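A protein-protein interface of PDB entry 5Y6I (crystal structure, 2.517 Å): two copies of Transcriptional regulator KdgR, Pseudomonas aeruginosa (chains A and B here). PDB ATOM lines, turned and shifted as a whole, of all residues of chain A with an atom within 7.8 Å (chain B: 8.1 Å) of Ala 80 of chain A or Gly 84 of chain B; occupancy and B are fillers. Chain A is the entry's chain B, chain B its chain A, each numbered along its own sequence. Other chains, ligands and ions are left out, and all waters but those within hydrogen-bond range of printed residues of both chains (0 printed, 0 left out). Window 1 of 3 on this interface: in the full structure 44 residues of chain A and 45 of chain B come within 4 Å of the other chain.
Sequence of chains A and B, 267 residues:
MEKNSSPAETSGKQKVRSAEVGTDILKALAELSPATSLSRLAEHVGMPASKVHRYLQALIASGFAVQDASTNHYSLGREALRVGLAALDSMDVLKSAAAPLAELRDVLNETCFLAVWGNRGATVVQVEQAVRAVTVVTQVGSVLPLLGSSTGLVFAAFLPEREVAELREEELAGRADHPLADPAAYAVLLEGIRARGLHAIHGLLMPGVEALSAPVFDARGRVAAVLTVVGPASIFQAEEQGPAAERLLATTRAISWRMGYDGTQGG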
ATOM      1  N   LEU A  26      17.412  16.903  17.154  1.00  0.00           N
ATOM      2  CA  LEU A  26      18.084  17.975  16.414  1.00  0.00           C
ATOM      3  C   LEU A  26      18.887  17.435  15.230  1.00  0.00           C
ATOM      4  O   LEU A  26      18.835  18.000  14.129  1.00  0.00           O
ATOM      5  CB  LEU A  26      19.005  18.772  17.341  1.00  0.00           C
ATOM      6  CG  LEU A  26      18.590  20.197  17.666  1.00  0.00           C
ATOM      7  CD1 LEU A  26      19.748  20.947  18.313  1.00  0.00           C
ATOM      8  CD2 LEU A  26      18.131  20.885  16.399  1.00  0.00           C
ATOM      9  N   ALA A  30      18.446  17.990  11.172  1.00  0.00           N
ATOM     10  CA  ALA A  30      19.450  18.470  10.225  1.00  0.00           C
ATOM     11  C   ALA A  30      19.579  17.528   9.033  1.00  0.00           C
ATOM     12  O   ALA A  30      19.522  17.965   7.876  1.00  0.00           O
ATOM     13  CB  ALA A  30      20.793  18.665  10.922  1.00  0.00           C
ATOM     14  N   SER A  62      13.052  26.442  22.749  1.00  0.00           N
ATOM     15  CA  SER A  62      14.451  26.845  22.666  1.00  0.00           C
ATOM     16  C   SER A  62      14.763  27.622  21.397  1.00  0.00           C
ATOM     17  O   SER A  62      15.788  28.308  21.351  1.00  0.00           O
ATOM     18  CB  SER A  62      15.368  25.615  22.721  1.00  0.00           C
ATOM     19  OG  SER A  62      15.403  25.025  24.014  1.00  0.00           O
ATOM     20  N   GLY A  63      13.933  27.509  20.361  1.00  0.00           N
ATOM     21  CA  GLY A  63      14.260  28.104  19.082  1.00  0.00           C
ATOM     22  C   GLY A  63      15.219  27.330  18.194  1.00  0.00           C
ATOM     23  O   GLY A  63      15.712  27.899  17.206  1.00  0.00           O
ATOM     24  N   PHE A  64      15.496  26.056  18.489  1.00  0.00           N
ATOM     25  CA  PHE A  64      16.284  25.212  17.592  1.00  0.00           C
ATOM     26  C   PHE A  64      15.435  24.529  16.532  1.00  0.00           C
ATOM     27  O   PHE A  64      15.980  23.832  15.672  1.00  0.00           O
ATOM     28  CB  PHE A  64      17.054  24.148  18.384  1.00  0.00           C
ATOM     29  CG  PHE A  64      18.206  24.700  19.161  1.00  0.00           C
ATOM     30  CD1 PHE A  64      19.458  24.787  18.602  1.00  0.00           C
ATOM     31  CD2 PHE A  64      18.032  25.157  20.451  1.00  0.00           C
ATOM     32  CE1 PHE A  64      20.522  25.329  19.321  1.00  0.00           C
ATOM     33  CE2 PHE A  64      19.092  25.682  21.172  1.00  0.00           C
ATOM     34  CZ  PHE A  64      20.334  25.767  20.599  1.00  0.00           C
ATOM     35  N   ALA A  65      14.119  24.705  16.573  1.00  0.00           N
ATOM     36  CA  ALA A  65      13.222  24.102  15.594  1.00  0.00           C
ATOM     37  C   ALA A  65      12.018  25.003  15.436  1.00  0.00           C
ATOM     38  O   ALA A  65      11.644  25.712  16.372  1.00  0.00           O
ATOM     39  CB  ALA A  65      12.783  22.691  16.016  1.00  0.00           C
ATOM     40  N   SER A  75      11.224  22.088  10.770  1.00  0.00           N
ATOM     41  CA  SER A  75      12.486  22.494  10.158  1.00  0.00           C
ATOM     42  C   SER A  75      13.366  23.122  11.229  1.00  0.00           C
ATOM     43  O   SER A  75      12.907  23.432  12.331  1.00  0.00           O
ATOM     44  CB  SER A  75      12.248  23.473   9.001  1.00  0.00           C
ATOM     45  OG  SER A  75      11.307  24.447   9.389  1.00  0.00           O
ATOM     46  N   LEU A  76      14.644  23.298  10.905  1.00  0.00           N
ATOM     47  CA  LEU A  76      15.573  23.790  11.912  1.00  0.00           C
ATOM     48  C   LEU A  76      15.235  25.229  12.274  1.00  0.00           C
ATOM     49  O   LEU A  76      14.723  25.994  11.450  1.00  0.00           O
ATOM     50  CB  LEU A  76      17.017  23.685  11.421  1.00  0.00           C
ATOM     51  CG  LEU A  76      17.685  22.325  11.532  1.00  0.00           C
ATOM     52  CD1 LEU A  76      19.116  22.420  11.015  1.00  0.00           C
ATOM     53  CD2 LEU A  76      17.633  21.796  12.986  1.00  0.00           C
ATOM     54  N   GLY A  77      15.515  25.588  13.536  1.00  0.00           N
ATOM     55  CA  GLY A  77      15.116  26.871  14.081  1.00  0.00           C
ATOM     56  C   GLY A  77      16.200  27.928  13.981  1.00  0.00           C
ATOM     57  O   GLY A  77      17.330  27.680  13.559  1.00  0.00           O
ATOM     58  N   ARG A  78      15.839  29.142  14.397  1.00  0.00           N
ATOM     59  CA  ARG A  78      16.764  30.267  14.296  1.00  0.00           C
ATOM     60  C   ARG A  78      18.018  30.038  15.140  1.00  0.00           C
ATOM     61  O   ARG A  78      19.120  30.430  14.740  1.00  0.00           O
ATOM     62  CB  ARG A  78      16.067  31.564  14.715  1.00  0.00           C
ATOM     63  CG  ARG A  78      17.057  32.636  15.117  1.00  0.00           C
ATOM     64  CD  ARG A  78      16.498  33.576  16.146  1.00  0.00           C
ATOM     65  NE  ARG A  78      17.529  34.402  16.785  1.00  0.00           N
ATOM     66  CZ  ARG A  78      18.214  35.372  16.179  1.00  0.00           C
ATOM     67  NH1 ARG A  78      17.998  35.639  14.902  1.00  0.00           N
ATOM     68  NH2 ARG A  78      19.123  36.081  16.843  1.00  0.00           N
ATOM     69  N   GLU A  79      17.872  29.396  16.305  1.00  0.00           N
ATOM     70  CA  GLU A  79      19.027  29.162  17.167  1.00  0.00           C
ATOM     71  C   GLU A  79      20.067  28.281  16.499  1.00  0.00           C
ATOM     72  O   GLU A  79      21.263  28.408  16.779  1.00  0.00           O
ATOM     73  CB  GLU A  79      18.570  28.547  18.485  1.00  0.00           C
ATOM     74  CG  GLU A  79      17.978  29.584  19.380  1.00  0.00           C
ATOM     75  CD  GLU A  79      18.865  30.810  19.455  1.00  0.00           C
ATOM     76  OE1 GLU A  79      20.086  30.641  19.671  1.00  0.00           O
ATOM     77  OE2 GLU A  79      18.348  31.936  19.279  1.00  0.00           O
ATOM     78  N   ALA A  80      19.631  27.389  15.620  1.00  0.00           N
ATOM     79  CA  ALA A  80      20.561  26.564  14.868  1.00  0.00           C
ATOM     80  C   ALA A  80      21.483  27.409  13.997  1.00  0.00           C
ATOM     81  O   ALA A  80      22.669  27.095  13.846  1.00  0.00           O
ATOM     82  CB  ALA A  80      19.776  25.567  14.018  1.00  0.00           C
ATOM     83  N   LEU A  81      20.959  28.477  13.392  1.00  0.00           N
ATOM     84  CA  LEU A  81      21.835  29.389  12.659  1.00  0.00           C
ATOM     85  C   LEU A  81      22.800  30.074  13.605  1.00  0.00           C
ATOM     86  O   LEU A  81      23.991  30.200  13.305  1.00  0.00           O
ATOM     87  CB  LEU A  81      21.029  30.441  11.903  1.00  0.00           C
ATOM     88  CG  LEU A  81      19.976  29.930  10.934  1.00  0.00           C
ATOM     89  CD1 LEU A  81      18.803  30.917  10.733  1.00  0.00           C
ATOM     90  CD2 LEU A  81      20.648  29.591   9.615  1.00  0.00           C
ATOM     91  N   ARG A  82      22.300  30.523  14.753  1.00  0.00           N
ATOM     92  CA  ARG A  82      23.181  31.120  15.750  1.00  0.00           C
ATOM     93  C   ARG A  82      24.331  30.182  16.087  1.00  0.00           C
ATOM     94  O   ARG A  82      25.496  30.592  16.112  1.00  0.00           O
ATOM     95  CB  ARG A  82      22.387  31.476  17.000  1.00  0.00           C
ATOM     96  CG  ARG A  82      21.171  32.271  16.661  1.00  0.00           C
ATOM     97  CD  ARG A  82      21.579  33.379  15.707  1.00  0.00           C
ATOM     98  NE  ARG A  82      22.359  34.398  16.394  1.00  0.00           N
ATOM     99  CZ  ARG A  82      23.256  35.175  15.802  1.00  0.00           C
ATOM    100  NH1 ARG A  82      23.903  36.091  16.502  1.00  0.00           N
ATOM    101  NH2 ARG A  82      23.518  35.021  14.515  1.00  0.00           N
ATOM    102  N   VAL A  83      24.017  28.904  16.307  1.00  0.00           N
ATOM    103  CA  VAL A  83      25.035  27.937  16.688  1.00  0.00           C
ATOM    104  C   VAL A  83      25.940  27.631  15.506  1.00  0.00           C
ATOM    105  O   VAL A  83      27.140  27.377  15.682  1.00  0.00           O
ATOM    106  CB  VAL A  83      24.363  26.668  17.253  1.00  0.00           C
ATOM    107  CG1 VAL A  83      25.344  25.500  17.331  1.00  0.00           C
ATOM    108  CG2 VAL A  83      23.750  26.950  18.629  1.00  0.00           C
ATOM    109  N   GLY A  84      25.403  27.659  14.284  1.00  0.00           N
ATOM    110  CA  GLY A  84      26.278  27.528  13.134  1.00  0.00           C
ATOM    111  C   GLY A  84      27.292  28.657  13.077  1.00  0.00           C
ATOM    112  O   GLY A  84      28.485  28.433  12.849  1.00  0.00           O
ATOM    113  N   LEU A  85      26.838  29.887  13.326  1.00  0.00           N
ATOM    114  CA  LEU A  85      27.724  31.022  13.140  1.00  0.00           C
ATOM    115  C   LEU A  85      28.714  31.141  14.289  1.00  0.00           C
ATOM    116  O   LEU A  85      29.891  31.451  14.063  1.00  0.00           O
ATOM    117  CB  LEU A  85      26.911  32.304  12.965  1.00  0.00           C
ATOM    118  CG  LEU A  85      26.037  32.267  11.710  1.00  0.00           C
ATOM    119  CD1 LEU A  85      25.274  33.559  11.545  1.00  0.00           C
ATOM    120  CD2 LEU A  85      26.884  31.986  10.457  1.00  0.00           C
ATOM    121  N   ALA A  86      28.266  30.869  15.519  1.00  0.00           N
ATOM    122  CA  ALA A  86      29.188  30.848  16.652  1.00  0.00           C
ATOM    123  C   ALA A  86      30.251  29.772  16.465  1.00  0.00           C
ATOM    124  O   ALA A  86      31.443  30.042  16.634  1.00  0.00           O
ATOM    125  CB  ALA A  86      28.430  30.637  17.964  1.00  0.00           C
ATOM    126  N   ALA A  87      29.840  28.547  16.094  1.00  0.00           N
ATOM    127  CA  ALA A  87      30.814  27.496  15.788  1.00  0.00           C
ATOM    128  C   ALA A  87      31.868  27.980  14.809  1.00  0.00           C
ATOM    129  O   ALA A  87      33.050  27.634  14.926  1.00  0.00           O
ATOM    130  CB  ALA A  87      30.125  26.267  15.205  1.00  0.00           C
ATOM    131  N   LEU A  88      31.461  28.775  13.823  1.00  0.00           N
ATOM    132  CA  LEU A  88      32.437  29.229  12.845  1.00  0.00           C
ATOM    133  C   LEU A  88      33.292  30.355  13.400  1.00  0.00           C
ATOM    134  O   LEU A  88      34.486  30.416  13.111  1.00  0.00           O
ATOM    135  CB  LEU A  88      31.737  29.665  11.567  1.00  0.00           C
ATOM    136  CG  LEU A  88      30.982  28.550  10.859  1.00  0.00           C
ATOM    137  CD1 LEU A  88      29.951  29.169   9.894  1.00  0.00           C
ATOM    138  CD2 LEU A  88      31.950  27.665  10.143  1.00  0.00           C
ATOM    139  N   VAL A 140      26.298  24.761   1.293  1.00  0.00           N
ATOM    140  CA  VAL A 140      26.974  24.953   2.570  1.00  0.00           C
ATOM    141  C   VAL A 140      26.726  23.721   3.432  1.00  0.00           C
ATOM    142  O   VAL A 140      25.601  23.209   3.503  1.00  0.00           O
ATOM    143  CB  VAL A 140      26.488  26.242   3.253  1.00  0.00           C
ATOM    144  CG1 VAL A 140      26.649  26.131   4.750  1.00  0.00           C
ATOM    145  CG2 VAL A 140      27.283  27.435   2.758  1.00  0.00           C
ATOM    146  N   GLY A 141      27.790  23.200   4.039  1.00  0.00           N
ATOM    147  CA  GLY A 141      27.673  22.013   4.869  1.00  0.00           C
ATOM    148  C   GLY A 141      27.815  20.697   4.139  1.00  0.00           C
ATOM    149  O   GLY A 141      27.605  19.645   4.749  1.00  0.00           O
ATOM    150  N   LEU B  26      23.271  24.629  25.221  1.00  0.00           N
ATOM    151  CA  LEU B  26      23.951  24.757  23.941  1.00  0.00           C
ATOM    152  C   LEU B  26      23.788  26.162  23.391  1.00  0.00           C
ATOM    153  O   LEU B  26      24.719  26.729  22.804  1.00  0.00           O
ATOM    154  CB  LEU B  26      23.409  23.719  22.967  1.00  0.00           C
ATOM    155  CG  LEU B  26      23.918  23.662  21.531  1.00  0.00           C
ATOM    156  CD1 LEU B  26      25.392  23.266  21.461  1.00  0.00           C
ATOM    157  CD2 LEU B  26      23.061  22.679  20.735  1.00  0.00           C
ATOM    158  N   LYS B  27      22.620  26.756  23.611  1.00  0.00           N
ATOM    159  CA  LYS B  27      22.369  28.093  23.107  1.00  0.00           C
ATOM    160  C   LYS B  27      23.242  29.113  23.820  1.00  0.00           C
ATOM    161  O   LYS B  27      23.679  30.101  23.217  1.00  0.00           O
ATOM    162  CB  LYS B  27      20.882  28.438  23.266  1.00  0.00           C
ATOM    163  CG  LYS B  27      20.526  29.868  22.907  1.00  0.00           C
ATOM    164  CD  LYS B  27      19.212  30.313  23.532  1.00  0.00           C
ATOM    165  CE  LYS B  27      18.020  29.634  22.874  1.00  0.00           C
ATOM    166  NZ  LYS B  27      16.715  30.245  23.272  1.00  0.00           N
ATOM    167  N   ALA B  30      27.030  28.799  22.585  1.00  0.00           N
ATOM    168  CA  ALA B  30      27.207  29.543  21.337  1.00  0.00           C
ATOM    169  C   ALA B  30      27.286  31.045  21.589  1.00  0.00           C
ATOM    170  O   ALA B  30      28.081  31.754  20.961  1.00  0.00           O
ATOM    171  CB  ALA B  30      26.059  29.230  20.381  1.00  0.00           C
ATOM    172  N   PHE B  64      28.238  17.767  20.676  1.00  0.00           N
ATOM    173  CA  PHE B  64      27.719  19.118  20.555  1.00  0.00           C
ATOM    174  C   PHE B  64      28.580  20.136  21.285  1.00  0.00           C
ATOM    175  O   PHE B  64      28.429  21.342  21.041  1.00  0.00           O
ATOM    176  CB  PHE B  64      26.260  19.169  21.047  1.00  0.00           C
ATOM    177  CG  PHE B  64      25.248  18.819  19.971  1.00  0.00           C
ATOM    178  CD1 PHE B  64      24.883  17.516  19.745  1.00  0.00           C
ATOM    179  CD2 PHE B  64      24.691  19.798  19.177  1.00  0.00           C
ATOM    180  CE1 PHE B  64      23.979  17.192  18.754  1.00  0.00           C
ATOM    181  CE2 PHE B  64      23.786  19.477  18.181  1.00  0.00           C
ATOM    182  CZ  PHE B  64      23.431  18.163  17.975  1.00  0.00           C
ATOM    183  N   GLY B  77      30.974  21.842  19.825  1.00  0.00           N
ATOM    184  CA  GLY B  77      31.520  20.706  19.119  1.00  0.00           C
ATOM    185  C   GLY B  77      31.182  20.725  17.638  1.00  0.00           C
ATOM    186  O   GLY B  77      30.471  21.598  17.129  1.00  0.00           O
ATOM    187  N   ARG B  78      31.716  19.722  16.936  1.00  0.00           N
ATOM    188  CA  ARG B  78      31.438  19.573  15.513  1.00  0.00           C
ATOM    189  C   ARG B  78      29.971  19.260  15.249  1.00  0.00           C
ATOM    190  O   ARG B  78      29.447  19.629  14.190  1.00  0.00           O
ATOM    191  CB  ARG B  78      32.318  18.484  14.911  1.00  0.00           C
ATOM    192  CG  ARG B  78      33.684  18.949  14.464  1.00  0.00           C
ATOM    193  CD  ARG B  78      33.618  20.121  13.506  1.00  0.00           C
ATOM    194  NE  ARG B  78      34.866  20.872  13.548  1.00  0.00           N
ATOM    195  CZ  ARG B  78      35.123  21.833  14.432  1.00  0.00           C
ATOM    196  NH1 ARG B  78      36.294  22.459  14.411  1.00  0.00           N
ATOM    197  NH2 ARG B  78      34.214  22.169  15.341  1.00  0.00           N
ATOM    198  N   GLU B  79      29.291  18.580  16.178  1.00  0.00           N
ATOM    199  CA  GLU B  79      27.848  18.413  16.025  1.00  0.00           C
ATOM    200  C   GLU B  79      27.131  19.755  16.033  1.00  0.00           C
ATOM    201  O   GLU B  79      26.162  19.955  15.293  1.00  0.00           O
ATOM    202  CB  GLU B  79      27.294  17.510  17.121  1.00  0.00           C
ATOM    203  CG  GLU B  79      27.414  16.050  16.786  1.00  0.00           C
ATOM    204  CD  GLU B  79      27.027  15.777  15.353  1.00  0.00           C
ATOM    205  OE1 GLU B  79      25.988  16.312  14.890  1.00  0.00           O
ATOM    206  OE2 GLU B  79      27.772  15.046  14.678  1.00  0.00           O
ATOM    207  N   ALA B  80      27.592  20.688  16.861  1.00  0.00           N
ATOM    208  CA  ALA B  80      27.034  22.031  16.824  1.00  0.00           C
ATOM    209  C   ALA B  80      27.243  22.660  15.454  1.00  0.00           C
ATOM    210  O   ALA B  80      26.338  23.304  14.909  1.00  0.00           O
ATOM    211  CB  ALA B  80      27.667  22.891  17.920  1.00  0.00           C
ATOM    212  N   LEU B  81      28.430  22.474  14.878  1.00  0.00           N
ATOM    213  CA  LEU B  81      28.712  23.057  13.575  1.00  0.00           C
ATOM    214  C   LEU B  81      27.852  22.428  12.483  1.00  0.00           C
ATOM    215  O   LEU B  81      27.359  23.127  11.595  1.00  0.00           O
ATOM    216  CB  LEU B  81      30.203  22.892  13.250  1.00  0.00           C
ATOM    217  CG  LEU B  81      30.665  23.249  11.835  1.00  0.00           C
ATOM    218  CD1 LEU B  81      30.302  24.678  11.497  1.00  0.00           C
ATOM    219  CD2 LEU B  81      32.166  23.010  11.666  1.00  0.00           C
ATOM    220  N   ARG B  82      27.666  21.110  12.516  1.00  0.00           N
ATOM    221  CA  ARG B  82      27.018  20.456  11.385  1.00  0.00           C
ATOM    222  C   ARG B  82      25.526  20.770  11.334  1.00  0.00           C
ATOM    223  O   ARG B  82      24.966  20.963  10.243  1.00  0.00           O
ATOM    224  CB  ARG B  82      27.259  18.958  11.438  1.00  0.00           C
ATOM    225  CG  ARG B  82      28.699  18.611  11.076  1.00  0.00           C
ATOM    226  CD  ARG B  82      29.041  17.153  11.291  1.00  0.00           C
ATOM    227  NE  ARG B  82      29.952  16.961  12.414  1.00  0.00           N
ATOM    228  CZ  ARG B  82      30.610  15.831  12.637  1.00  0.00           C
ATOM    229  NH1 ARG B  82      31.424  15.719  13.685  1.00  0.00           N
ATOM    230  NH2 ARG B  82      30.449  14.809  11.805  1.00  0.00           N
ATOM    231  N   VAL B  83      24.865  20.820  12.498  1.00  0.00           N
ATOM    232  CA  VAL B  83      23.472  21.261  12.553  1.00  0.00           C
ATOM    233  C   VAL B  83      23.356  22.690  12.045  1.00  0.00           C
ATOM    234  O   VAL B  83      22.487  23.016  11.219  1.00  0.00           O
ATOM    235  CB  VAL B  83      22.921  21.135  13.986  1.00  0.00           C
ATOM    236  CG1 VAL B  83      21.611  21.935  14.145  1.00  0.00           C
ATOM    237  CG2 VAL B  83      22.734  19.672  14.365  1.00  0.00           C
ATOM    238  N   GLY B  84      24.238  23.563  12.543  1.00  0.00           N
ATOM    239  CA  GLY B  84      24.218  24.956  12.135  1.00  0.00           C
ATOM    240  C   GLY B  84      24.410  25.145  10.643  1.00  0.00           C
ATOM    241  O   GLY B  84      23.728  25.966  10.025  1.00  0.00           O
ATOM    242  N   LEU B  85      25.329  24.386  10.041  1.00  0.00           N
ATOM    243  CA  LEU B  85      25.524  24.509   8.597  1.00  0.00           C
ATOM    244  C   LEU B  85      24.334  23.967   7.821  1.00  0.00           C
ATOM    245  O   LEU B  85      24.091  24.394   6.682  1.00  0.00           O
ATOM    246  CB  LEU B  85      26.794  23.787   8.145  1.00  0.00           C
ATOM    247  CG  LEU B  85      28.164  24.256   8.651  1.00  0.00           C
ATOM    248  CD1 LEU B  85      29.238  23.301   8.141  1.00  0.00           C
ATOM    249  CD2 LEU B  85      28.484  25.695   8.255  1.00  0.00           C
ATOM    250  N   ALA B  86      23.622  22.991   8.386  1.00  0.00           N
ATOM    251  CA  ALA B  86      22.382  22.538   7.775  1.00  0.00           C
ATOM    252  C   ALA B  86      21.354  23.657   7.797  1.00  0.00           C
ATOM    253  O   ALA B  86      20.675  23.910   6.793  1.00  0.00           O
ATOM    254  CB  ALA B  86      21.841  21.307   8.506  1.00  0.00           C
ATOM    255  N   ALA B  87      21.261  24.361   8.930  1.00  0.00           N
ATOM    256  CA  ALA B  87      20.388  25.520   9.037  1.00  0.00           C
ATOM    257  C   ALA B  87      20.730  26.556   7.982  1.00  0.00           C
ATOM    258  O   ALA B  87      19.871  26.977   7.204  1.00  0.00           O
ATOM    259  CB  ALA B  87      20.498  26.129  10.439  1.00  0.00           C
ATOM    260  N   LEU B  88      21.999  26.970   7.936  1.00  0.00           N
ATOM    261  CA  LEU B  88      22.419  28.020   7.009  1.00  0.00           C
ATOM    262  C   LEU B  88      22.212  27.606   5.552  1.00  0.00           C
ATOM    263  O   LEU B  88      21.926  28.447   4.694  1.00  0.00           O
ATOM    264  CB  LEU B  88      23.882  28.384   7.281  1.00  0.00           C
ATOM    265  CG  LEU B  88      24.152  29.002   8.661  1.00  0.00           C
ATOM    266  CD1 LEU B  88      25.574  28.762   9.071  1.00  0.00           C
ATOM    267  CD2 LEU B  88      23.886  30.499   8.656  1.00  0.00           C
ATOM    268  N   ASP B  89      22.366  26.318   5.245  1.00  0.00           N
ATOM    269  CA  ASP B  89      22.009  25.842   3.913  1.00  0.00           C
ATOM    270  C   ASP B  89      20.505  25.885   3.676  1.00  0.00           C
ATOM    271  O   ASP B  89      20.065  25.728   2.534  1.00  0.00           O
ATOM    272  CB  ASP B  89      22.511  24.406   3.709  1.00  0.00           C
ATOM    273  CG  ASP B  89      22.300  23.911   2.292  1.00  0.00           C
ATOM    274  OD1 ASP B  89      22.370  24.759   1.382  1.00  0.00           O
ATOM    275  OD2 ASP B  89      22.058  22.697   2.070  1.00  0.00           O
ATOM    276  N   SER B  90      19.704  26.074   4.720  1.00  0.00           N
ATOM    277  CA  SER B  90      18.259  26.047   4.569  1.00  0.00           C
ATOM    278  C   SER B  90      17.620  27.430   4.541  1.00  0.00           C
ATOM    279  O   SER B  90      16.426  27.525   4.244  1.00  0.00           O
ATOM    280  CB  SER B  90      17.628  25.229   5.693  1.00  0.00           C
ATOM    281  OG  SER B  90      18.001  23.873   5.601  1.00  0.00           O
ATOM    282  N   MET B  91      18.367  28.493   4.841  1.00  0.00           N
ATOM    283  CA  MET B  91      17.804  29.837   4.799  1.00  0.00           C
ATOM    284  C   MET B  91      17.121  30.090   3.459  1.00  0.00           C
ATOM    285  O   MET B  91      17.601  29.659   2.407  1.00  0.00           O
ATOM    286  CB  MET B  91      18.900  30.875   5.029  1.00  0.00           C
ATOM    287  CG  MET B  91      19.350  31.058   6.453  1.00  0.00           C
ATOM    288  SD  MET B  91      20.501  32.447   6.595  1.00  0.00           S
ATOM    289  CE  MET B  91      21.876  31.851   5.625  1.00  0.00           C
ATOM    290  N   ALA B 219      21.259  35.529   8.128  1.00  0.00           N
ATOM    291  CA  ALA B 219      22.090  35.249   9.292  1.00  0.00           C
ATOM    292  C   ALA B 219      23.435  35.951   9.213  1.00  0.00           C
ATOM    293  O   ALA B 219      23.937  36.460  10.223  1.00  0.00           O
ATOM    294  CB  ALA B 219      22.295  33.739   9.423  1.00  0.00           C
ATOM    295  N   GLY B 260      18.125  34.473  11.426  1.00  0.00           N
ATOM    296  CA  GLY B 260      19.331  34.339  12.207  1.00  0.00           C
ATOM    297  C   GLY B 260      20.089  35.620  12.407  1.00  0.00           C
ATOM    298  O   GLY B 260      21.084  35.631  13.144  1.00  0.00           O
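Among the printed residues, no Asp or Glu carboxylate lies within 4 Å of a Lys or Arg side-chain nitrogen of the other chain.
O of Ala 86 of chain B lies within hydrogen-bond range of OG of Ser 90 of chain B.
The side-chain sulfur (SD) of Met 91 of chain B sits at hydrogen-bond distance from the backbone NH (N) of Ala 219 of chain B (3.5 Å).
The backbone NH of Arg 78 of chain A lies within hydrogen-bond range of the backbone carbonyl oxygen of Gly 63 of chain A (3.1 Å).
The backbone carbonyl oxygen of Gly 63 of chain A sits at hydrogen-bond distance from the backbone NH of Glu 79 of chain A, at 2.8 Å.
Among the printed residues, pairs that only touch across the chains: Ala 30 of chain A with Ala 86 of chain B, Phe 64 of chain A with Leu 26 of chain B, Phe 64 of chain A with Lys 27 of chain B, Leu 76 of chain A with Val 83 of chain B, Leu 76 of chain A with Ala 86 of chain B, Leu 76 of chain A with Ala 87 of chain B, Arg 78 of chain A with Gly 260 of chain B, Glu 79 of chain A with Lys 27 of chain B, Ala 80 of chain A with Gly 84 of chain B, Ala 80 of chain A with Ala 87 of chain B, Leu 81 of chain A with Ala 87 of chain B, Leu 81 of chain A with Leu 88 of chain B, Leu 81 of chain A with Met 91 of chain B, Leu 81 of chain A with Gly 260 of chain B, Val 83 of chain A with Ala 30 of chain B, Val 83 of chain A with Ala 80 of chain B, Gly 84 of chain A with Gly 84 of chain B, Leu 85 of chain A with Leu 88 of chain B, Leu 85 of chain A with Ala 219 of chain B, Ala 86 of chain A with Ala 30 of chain B, Ala 87 of chain A with Leu 81 of chain B, Leu 88 of chain A with Leu 81 of chain B, Val 140 of chain A with Leu 85 of chain B, Val 140 of chain A with Asp 89 of chain B and Gly 141 of chain A with Leu 85 of chain B.
O of Ser 62 of chain A sits at hydrogen-bond distance from NZ of Lys 27 of chain B, at 2.9 Å.
The backbone carbonyl oxygen of Gly 260 of chain B is in hydrogen-bond range of the guanidinium group of Arg 82 of chain A, 2.9 Å away.
Printed residues of chain B within 4 Å of Phe 64 of chain A: Leu 26 and Lys 27.
Ala 80 of chain A touches just these residues of chain B: Gly 84 and Ala 87.
Printed residues of chain B within 4 Å of Ala 87 of chain A: Leu 81 (3.9 Å).
Of the printed residues of chain B, Val 140 of chain A touches Leu 85 and Asp 89.
Printed residues of chain B within 4 Å of Gly 141 of chain A: Leu 85.
Of the printed residues of chain A, Val 83 of chain B touches Leu 76.
Of chain A, only Ala 80 (3.1 Å) and Gly 84 (3.4 Å) come within 4 Å of Gly 84 of chain B.
The nearest printed residue of chain A that does not touch Lys 27 of chain B is Val 83 of chain A (4.8 Å).
Ala 80 of chain A touches Ala 87 of chain B, but with the chains exchanged Ala 87 of chain A does not touch Ala 80 of chain B (4.6 Å).
Leu 81 of chain A touches Leu 88 of chain B, and with the chains exchanged Leu 88 of chain A touches Leu 81 of chain B.
Val 83 of chain A touches Ala 30 of chain B, but with the chains exchanged Ala 30 of chain A does not touch Val 83 of chain B (4.1 Å).
15 positions are printed for both chains.
Of the 27 pairs that touch across the chains among the printed residues, 7 have their exchanged pair printed and touching as well.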
